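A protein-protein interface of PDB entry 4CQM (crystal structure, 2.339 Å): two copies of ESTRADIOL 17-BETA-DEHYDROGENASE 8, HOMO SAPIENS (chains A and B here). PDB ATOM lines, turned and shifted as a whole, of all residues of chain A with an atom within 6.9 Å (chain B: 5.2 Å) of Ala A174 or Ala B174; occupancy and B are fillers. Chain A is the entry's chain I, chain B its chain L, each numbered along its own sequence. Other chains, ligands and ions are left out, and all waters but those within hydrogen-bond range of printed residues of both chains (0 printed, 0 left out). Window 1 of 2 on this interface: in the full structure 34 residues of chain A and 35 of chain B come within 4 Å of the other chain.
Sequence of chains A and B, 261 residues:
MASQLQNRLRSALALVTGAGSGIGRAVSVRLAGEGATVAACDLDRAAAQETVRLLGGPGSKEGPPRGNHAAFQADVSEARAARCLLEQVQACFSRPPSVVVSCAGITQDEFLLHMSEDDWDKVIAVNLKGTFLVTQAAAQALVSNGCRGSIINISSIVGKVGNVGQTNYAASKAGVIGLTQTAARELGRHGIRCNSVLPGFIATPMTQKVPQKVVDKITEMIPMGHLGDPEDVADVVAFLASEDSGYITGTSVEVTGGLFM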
ATOM      1  N   LEU A 128       4.177 -31.182   6.368  1.00  0.00           N
ATOM      2  CA  LEU A 128       4.182 -30.471   7.643  1.00  0.00           C
ATOM      3  C   LEU A 128       2.879 -30.663   8.417  1.00  0.00           C
ATOM      4  O   LEU A 128       2.888 -31.185   9.533  1.00  0.00           O
ATOM      5  CB  LEU A 128       4.442 -28.978   7.421  1.00  0.00           C
ATOM      6  CG  LEU A 128       4.514 -28.113   8.679  1.00  0.00           C
ATOM      7  CD1 LEU A 128       5.604 -28.617   9.612  1.00  0.00           C
ATOM      8  CD2 LEU A 128       4.744 -26.654   8.317  1.00  0.00           C
ATOM      9  N   SER A 155      11.996 -36.387   8.852  1.00  0.00           N
ATOM     10  CA  SER A 155      12.288 -35.084   8.272  1.00  0.00           C
ATOM     11  C   SER A 155      13.208 -35.256   7.068  1.00  0.00           C
ATOM     12  O   SER A 155      12.958 -36.099   6.207  1.00  0.00           O
ATOM     13  CB  SER A 155      12.926 -34.160   9.311  1.00  0.00           C
ATOM     14  OG  SER A 155      13.204 -32.886   8.757  1.00  0.00           O
ATOM     15  N   SER A 156      14.270 -34.460   7.021  1.00  0.00           N
ATOM     16  CA  SER A 156      15.273 -34.566   5.967  1.00  0.00           C
ATOM     17  C   SER A 156      16.502 -33.739   6.320  1.00  0.00           C
ATOM     18  O   SER A 156      16.438 -32.854   7.173  1.00  0.00           O
ATOM     19  CB  SER A 156      14.706 -34.108   4.621  1.00  0.00           C
ATOM     20  OG  SER A 156      15.664 -34.259   3.587  1.00  0.00           O
ATOM     21  N   VAL A 158      17.636 -31.795   4.279  1.00  0.00           N
ATOM     22  CA  VAL A 158      17.225 -30.549   3.648  1.00  0.00           C
ATOM     23  C   VAL A 158      16.597 -29.618   4.682  1.00  0.00           C
ATOM     24  O   VAL A 158      16.713 -28.396   4.590  1.00  0.00           O
ATOM     25  CB  VAL A 158      16.223 -30.809   2.501  1.00  0.00           C
ATOM     26  CG1 VAL A 158      15.834 -29.512   1.816  1.00  0.00           C
ATOM     27  CG2 VAL A 158      16.813 -31.789   1.497  1.00  0.00           C
ATOM     28  N   GLY A 159      15.948 -30.207   5.680  1.00  0.00           N
ATOM     29  CA  GLY A 159      15.301 -29.443   6.731  1.00  0.00           C
ATOM     30  C   GLY A 159      16.274 -28.757   7.670  1.00  0.00           C
ATOM     31  O   GLY A 159      15.864 -28.025   8.571  1.00  0.00           O
ATOM     32  N   LYS A 160      17.566 -28.990   7.466  1.00  0.00           N
ATOM     33  CA  LYS A 160      18.589 -28.377   8.303  1.00  0.00           C
ATOM     34  C   LYS A 160      19.408 -27.344   7.530  1.00  0.00           C
ATOM     35  O   LYS A 160      19.884 -26.365   8.105  1.00  0.00           O
ATOM     36  CB  LYS A 160      19.518 -29.445   8.886  1.00  0.00           C
ATOM     37  CG  LYS A 160      20.434 -28.930   9.986  1.00  0.00           C
ATOM     38  CD  LYS A 160      21.462 -29.970  10.406  1.00  0.00           C
ATOM     39  CE  LYS A 160      22.484 -30.216   9.306  1.00  0.00           C
ATOM     40  NZ  LYS A 160      23.564 -31.144   9.746  1.00  0.00           N
ATOM     41  N   TYR A 169       9.710 -27.644   0.307  1.00  0.00           N
ATOM     42  CA  TYR A 169      10.133 -28.900   0.916  1.00  0.00           C
ATOM     43  C   TYR A 169      10.997 -28.666   2.153  1.00  0.00           C
ATOM     44  O   TYR A 169      10.795 -29.302   3.187  1.00  0.00           O
ATOM     45  CB  TYR A 169      10.890 -29.752  -0.104  1.00  0.00           C
ATOM     46  CG  TYR A 169      11.266 -31.131   0.392  1.00  0.00           C
ATOM     47  CD1 TYR A 169      10.361 -32.183   0.329  1.00  0.00           C
ATOM     48  CD2 TYR A 169      12.530 -31.384   0.913  1.00  0.00           C
ATOM     49  CE1 TYR A 169      10.700 -33.447   0.776  1.00  0.00           C
ATOM     50  CE2 TYR A 169      12.878 -32.645   1.363  1.00  0.00           C
ATOM     51  CZ  TYR A 169      11.960 -33.672   1.292  1.00  0.00           C
ATOM     52  OH  TYR A 169      12.302 -34.929   1.737  1.00  0.00           O
ATOM     53  N   ALA A 170      11.959 -27.753   2.040  1.00  0.00           N
ATOM     54  CA  ALA A 170      12.863 -27.451   3.145  1.00  0.00           C
ATOM     55  C   ALA A 170      12.116 -26.831   4.319  1.00  0.00           C
ATOM     56  O   ALA A 170      12.359 -27.184   5.472  1.00  0.00           O
ATOM     57  CB  ALA A 170      13.979 -26.524   2.686  1.00  0.00           C
ATOM     58  N   ALA A 171      11.212 -25.905   4.017  1.00  0.00           N
ATOM     59  CA  ALA A 171      10.417 -25.242   5.045  1.00  0.00           C
ATOM     60  C   ALA A 171       9.553 -26.248   5.796  1.00  0.00           C
ATOM     61  O   ALA A 171       9.398 -26.161   7.014  1.00  0.00           O
ATOM     62  CB  ALA A 171       9.553 -24.153   4.429  1.00  0.00           C
ATOM     63  N   SER A 172       8.996 -27.203   5.060  1.00  0.00           N
ATOM     64  CA  SER A 172       8.158 -28.236   5.653  1.00  0.00           C
ATOM     65  C   SER A 172       8.975 -29.160   6.550  1.00  0.00           C
ATOM     66  O   SER A 172       8.592 -29.431   7.688  1.00  0.00           O
ATOM     67  CB  SER A 172       7.457 -29.049   4.562  1.00  0.00           C
ATOM     68  OG  SER A 172       8.399 -29.672   3.708  1.00  0.00           O
ATOM     69  N   LYS A 173      10.105 -29.634   6.033  1.00  0.00           N
ATOM     70  CA  LYS A 173      10.959 -30.558   6.769  1.00  0.00           C
ATOM     71  C   LYS A 173      11.596 -29.897   7.987  1.00  0.00           C
ATOM     72  O   LYS A 173      11.778 -30.536   9.023  1.00  0.00           O
ATOM     73  CB  LYS A 173      12.044 -31.126   5.854  1.00  0.00           C
ATOM     74  CG  LYS A 173      11.504 -32.049   4.781  1.00  0.00           C
ATOM     75  CD  LYS A 173      10.735 -33.202   5.401  1.00  0.00           C
ATOM     76  CE  LYS A 173       9.981 -33.987   4.347  1.00  0.00           C
ATOM     77  NZ  LYS A 173       9.326 -35.198   4.913  1.00  0.00           N
ATOM     78  N   ALA A 174      11.935 -28.619   7.856  1.00  0.00           N
ATOM     79  CA  ALA A 174      12.477 -27.860   8.975  1.00  0.00           C
ATOM     80  C   ALA A 174      11.402 -27.671  10.038  1.00  0.00           C
ATOM     81  O   ALA A 174      11.691 -27.669  11.234  1.00  0.00           O
ATOM     82  CB  ALA A 174      13.008 -26.519   8.508  1.00  0.00           C
ATOM     83  N   GLY A 175      10.161 -27.517   9.589  1.00  0.00           N
ATOM     84  CA  GLY A 175       9.032 -27.378  10.491  1.00  0.00           C
ATOM     85  C   GLY A 175       8.793 -28.643  11.291  1.00  0.00           C
ATOM     86  O   GLY A 175       8.398 -28.582  12.455  1.00  0.00           O
ATOM     87  N   VAL A 176       9.034 -29.788  10.661  1.00  0.00           N
ATOM     88  CA  VAL A 176       8.894 -31.083  11.318  1.00  0.00           C
ATOM     89  C   VAL A 176       9.828 -31.182  12.522  1.00  0.00           C
ATOM     90  O   VAL A 176       9.461 -31.726  13.566  1.00  0.00           O
ATOM     91  CB  VAL A 176       9.186 -32.242  10.340  1.00  0.00           C
ATOM     92  CG1 VAL A 176       9.197 -33.576  11.068  1.00  0.00           C
ATOM     93  CG2 VAL A 176       8.166 -32.256   9.212  1.00  0.00           C
ATOM     94  N   ILE A 177      11.031 -30.639  12.371  1.00  0.00           N
ATOM     95  CA  ILE A 177      12.021 -30.652  13.440  1.00  0.00           C
ATOM     96  C   ILE A 177      11.566 -29.813  14.632  1.00  0.00           C
ATOM     97  O   ILE A 177      11.610 -30.271  15.774  1.00  0.00           O
ATOM     98  CB  ILE A 177      13.384 -30.138  12.944  1.00  0.00           C
ATOM     99  CG1 ILE A 177      13.870 -30.985  11.766  1.00  0.00           C
ATOM    100  CG2 ILE A 177      14.403 -30.154  14.071  1.00  0.00           C
ATOM    101  CD1 ILE A 177      15.204 -30.548  11.204  1.00  0.00           C
ATOM    102  N   GLY A 178      11.127 -28.588  14.363  1.00  0.00           N
ATOM    103  CA  GLY A 178      10.623 -27.713  15.407  1.00  0.00           C
ATOM    104  C   GLY A 178       9.348 -28.254  16.024  1.00  0.00           C
ATOM    105  O   GLY A 178       9.050 -28.004  17.193  1.00  0.00           O
ATOM    106  N   LEU A 179       8.593 -29.002  15.227  1.00  0.00           N
ATOM    107  CA  LEU A 179       7.362 -29.631  15.686  1.00  0.00           C
ATOM    108  C   LEU A 179       7.658 -30.783  16.639  1.00  0.00           C
ATOM    109  O   LEU A 179       7.072 -30.880  17.716  1.00  0.00           O
ATOM    110  CB  LEU A 179       6.548 -30.128  14.487  1.00  0.00           C
ATOM    111  CG  LEU A 179       5.177 -30.766  14.703  1.00  0.00           C
ATOM    112  CD1 LEU A 179       4.296 -30.438  13.518  1.00  0.00           C
ATOM    113  CD2 LEU A 179       5.280 -32.274  14.870  1.00  0.00           C
ATOM    114  N   GLN A 181      10.378 -31.391  18.305  1.00  0.00           N
ATOM    115  CA  GLN A 181      11.035 -30.889  19.507  1.00  0.00           C
ATOM    116  C   GLN A 181      10.016 -30.403  20.532  1.00  0.00           C
ATOM    117  O   GLN A 181      10.204 -30.573  21.737  1.00  0.00           O
ATOM    118  CB  GLN A 181      12.005 -29.760  19.155  1.00  0.00           C
ATOM    119  CG  GLN A 181      13.280 -30.224  18.471  1.00  0.00           C
ATOM    120  CD  GLN A 181      14.086 -29.073  17.903  1.00  0.00           C
ATOM    121  OE1 GLN A 181      13.530 -28.047  17.508  1.00  0.00           O
ATOM    122  NE2 GLN A 181      15.403 -29.235  17.861  1.00  0.00           N
ATOM    123  N   SER B 155      12.666 -14.926  12.521  1.00  0.00           N
ATOM    124  CA  SER B 155      12.226 -16.203  13.067  1.00  0.00           C
ATOM    125  C   SER B 155      12.120 -16.131  14.589  1.00  0.00           C
ATOM    126  O   SER B 155      11.607 -15.153  15.138  1.00  0.00           O
ATOM    127  CB  SER B 155      13.186 -17.320  12.651  1.00  0.00           C
ATOM    128  OG  SER B 155      12.773 -18.573  13.167  1.00  0.00           O
ATOM    129  N   GLY B 159      12.152 -21.650  17.173  1.00  0.00           N
ATOM    130  CA  GLY B 159      12.306 -22.391  15.935  1.00  0.00           C
ATOM    131  C   GLY B 159      13.444 -23.398  15.969  1.00  0.00           C
ATOM    132  O   GLY B 159      13.478 -24.330  15.166  1.00  0.00           O
ATOM    133  N   TYR B 169       3.670 -22.586  16.435  1.00  0.00           N
ATOM    134  CA  TYR B 169       4.599 -21.465  16.403  1.00  0.00           C
ATOM    135  C   TYR B 169       6.020 -21.937  16.117  1.00  0.00           C
ATOM    136  O   TYR B 169       6.733 -21.331  15.317  1.00  0.00           O
ATOM    137  CB  TYR B 169       4.551 -20.695  17.724  1.00  0.00           C
ATOM    138  CG  TYR B 169       5.431 -19.465  17.753  1.00  0.00           C
ATOM    139  CD1 TYR B 169       5.008 -18.274  17.178  1.00  0.00           C
ATOM    140  CD2 TYR B 169       6.681 -19.494  18.358  1.00  0.00           C
ATOM    141  CE1 TYR B 169       5.807 -17.147  17.202  1.00  0.00           C
ATOM    142  CE2 TYR B 169       7.487 -18.372  18.387  1.00  0.00           C
ATOM    143  CZ  TYR B 169       7.044 -17.200  17.807  1.00  0.00           C
ATOM    144  OH  TYR B 169       7.840 -16.079  17.833  1.00  0.00           O
ATOM    145  N   ALA B 170       6.426 -23.020  16.772  1.00  0.00           N
ATOM    146  CA  ALA B 170       7.763 -23.570  16.584  1.00  0.00           C
ATOM    147  C   ALA B 170       7.939 -24.116  15.172  1.00  0.00           C
ATOM    148  O   ALA B 170       8.988 -23.940  14.558  1.00  0.00           O
ATOM    149  CB  ALA B 170       8.044 -24.659  17.607  1.00  0.00           C
ATOM    150  N   ALA B 171       6.904 -24.781  14.665  1.00  0.00           N
ATOM    151  CA  ALA B 171       6.943 -25.356  13.325  1.00  0.00           C
ATOM    152  C   ALA B 171       7.100 -24.269  12.270  1.00  0.00           C
ATOM    153  O   ALA B 171       7.904 -24.398  11.346  1.00  0.00           O
ATOM    154  CB  ALA B 171       5.687 -26.173  13.062  1.00  0.00           C
ATOM    155  N   SER B 172       6.327 -23.197  12.418  1.00  0.00           N
ATOM    156  CA  SER B 172       6.384 -22.074  11.491  1.00  0.00           C
ATOM    157  C   SER B 172       7.762 -21.420  11.504  1.00  0.00           C
ATOM    158  O   SER B 172       8.380 -21.239  10.456  1.00  0.00           O
ATOM    159  CB  SER B 172       5.308 -21.042  11.835  1.00  0.00           C
ATOM    160  OG  SER B 172       5.499 -20.526  13.141  1.00  0.00           O
ATOM    161  N   LYS B 173       8.237 -21.078  12.699  1.00  0.00           N
ATOM    162  CA  LYS B 173       9.527 -20.413  12.857  1.00  0.00           C
ATOM    163  C   LYS B 173      10.680 -21.271  12.358  1.00  0.00           C
ATOM    164  O   LYS B 173      11.619 -20.763  11.744  1.00  0.00           O
ATOM    165  CB  LYS B 173       9.753 -20.037  14.322  1.00  0.00           C
ATOM    166  CG  LYS B 173       8.821 -18.953  14.815  1.00  0.00           C
ATOM    167  CD  LYS B 173       8.920 -17.722  13.934  1.00  0.00           C
ATOM    168  CE  LYS B 173       7.914 -16.673  14.349  1.00  0.00           C
ATOM    169  NZ  LYS B 173       8.072 -15.406  13.581  1.00  0.00           N
ATOM    170  N   ALA B 174      10.608 -22.571  12.624  1.00  0.00           N
ATOM    171  CA  ALA B 174      11.611 -23.501  12.127  1.00  0.00           C
ATOM    172  C   ALA B 174      11.543 -23.565  10.608  1.00  0.00           C
ATOM    173  O   ALA B 174      12.567 -23.664   9.933  1.00  0.00           O
ATOM    174  CB  ALA B 174      11.412 -24.878  12.730  1.00  0.00           C
ATOM    175  N   GLY B 175      10.326 -23.497  10.080  1.00  0.00           N
ATOM    176  CA  GLY B 175      10.113 -23.491   8.645  1.00  0.00           C
ATOM    177  C   GLY B 175      10.658 -22.234   7.995  1.00  0.00           C
ATOM    178  O   GLY B 175      11.118 -22.269   6.855  1.00  0.00           O
ATOM    179  N   VAL B 176      10.597 -21.123   8.723  1.00  0.00           N
ATOM    180  CA  VAL B 176      11.130 -19.852   8.245  1.00  0.00           C
ATOM    181  C   VAL B 176      12.631 -19.953   7.990  1.00  0.00           C
ATOM    182  O   VAL B 176      13.138 -19.446   6.988  1.00  0.00           O
ATOM    183  CB  VAL B 176      10.855 -18.711   9.254  1.00  0.00           C
ATOM    184  CG1 VAL B 176      11.629 -17.456   8.877  1.00  0.00           C
ATOM    185  CG2 VAL B 176       9.364 -18.419   9.334  1.00  0.00           C
ATOM    186  N   ILE B 177      13.333 -20.624   8.897  1.00  0.00           N
ATOM    187  CA  ILE B 177      14.778 -20.786   8.788  1.00  0.00           C
ATOM    188  C   ILE B 177      15.162 -21.562   7.532  1.00  0.00           C
ATOM    189  O   ILE B 177      15.986 -21.103   6.741  1.00  0.00           O
ATOM    190  CB  ILE B 177      15.355 -21.502  10.022  1.00  0.00           C
ATOM    191  CG1 ILE B 177      15.035 -20.709  11.292  1.00  0.00           C
ATOM    192  CG2 ILE B 177      16.856 -21.694   9.873  1.00  0.00           C
ATOM    193  CD1 ILE B 177      15.603 -21.321  12.554  1.00  0.00           C
ATOM    194  N   GLY B 178      14.558 -22.733   7.350  1.00  0.00           N
ATOM    195  CA  GLY B 178      14.816 -23.552   6.178  1.00  0.00           C
ATOM    196  C   GLY B 178      14.402 -22.849   4.899  1.00  0.00           C
ATOM    197  O   GLY B 178      15.016 -23.028   3.847  1.00  0.00           O
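Of the printed residues of chain B, Ala A171 touches Gly B175 (3.2 Å).
Ala A174 touches just one residue of chain B: Ala B174 (3.2 Å).
Of the printed residues of chain A, Ala B171 touches Gly A175.
The nearest printed residue of chain B that does not touch Ala A174 is Gly B178 (4.2 Å).
The nearest printed residue of chain A that does not touch Ala B170 is Leu A179 (4.9 Å).
Hydrophobic or aromatic side chains of chain B that line the printed part of chain A: Ala B170, Ala B171 and Ala B174.
Among the printed residues, no Asp or Glu carboxylate lies within 4 Å of a Lys or Arg side-chain nitrogen of the other chain.
Among the printed residues, merely in contact across the chains: Ala A170 with Gly B178 (3.8 Å), Ala A171 with Gly B175 (3.2 Å), Ala A174 with Ala B174 (3.2 Å), Gly A175 with Ala B171 (3.3 Å), Gly A178 with Ala B170 (3.5 Å) and Gly A178 with Ala B174 (3.98 Å).
Ala A170 touches Gly B178, and with the chains exchanged Gly A178 touches Ala B170.
Ala A171 touches Gly B175, and with the chains exchanged Gly A175 touches Ala B171.
Ala B174 touches its own counterpart, Ala A174.
Gly A178 touches Ala B174, but with the chains exchanged Ala A174 does not touch Gly B178 (4.2 Å).
12 positions are printed for both chains.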
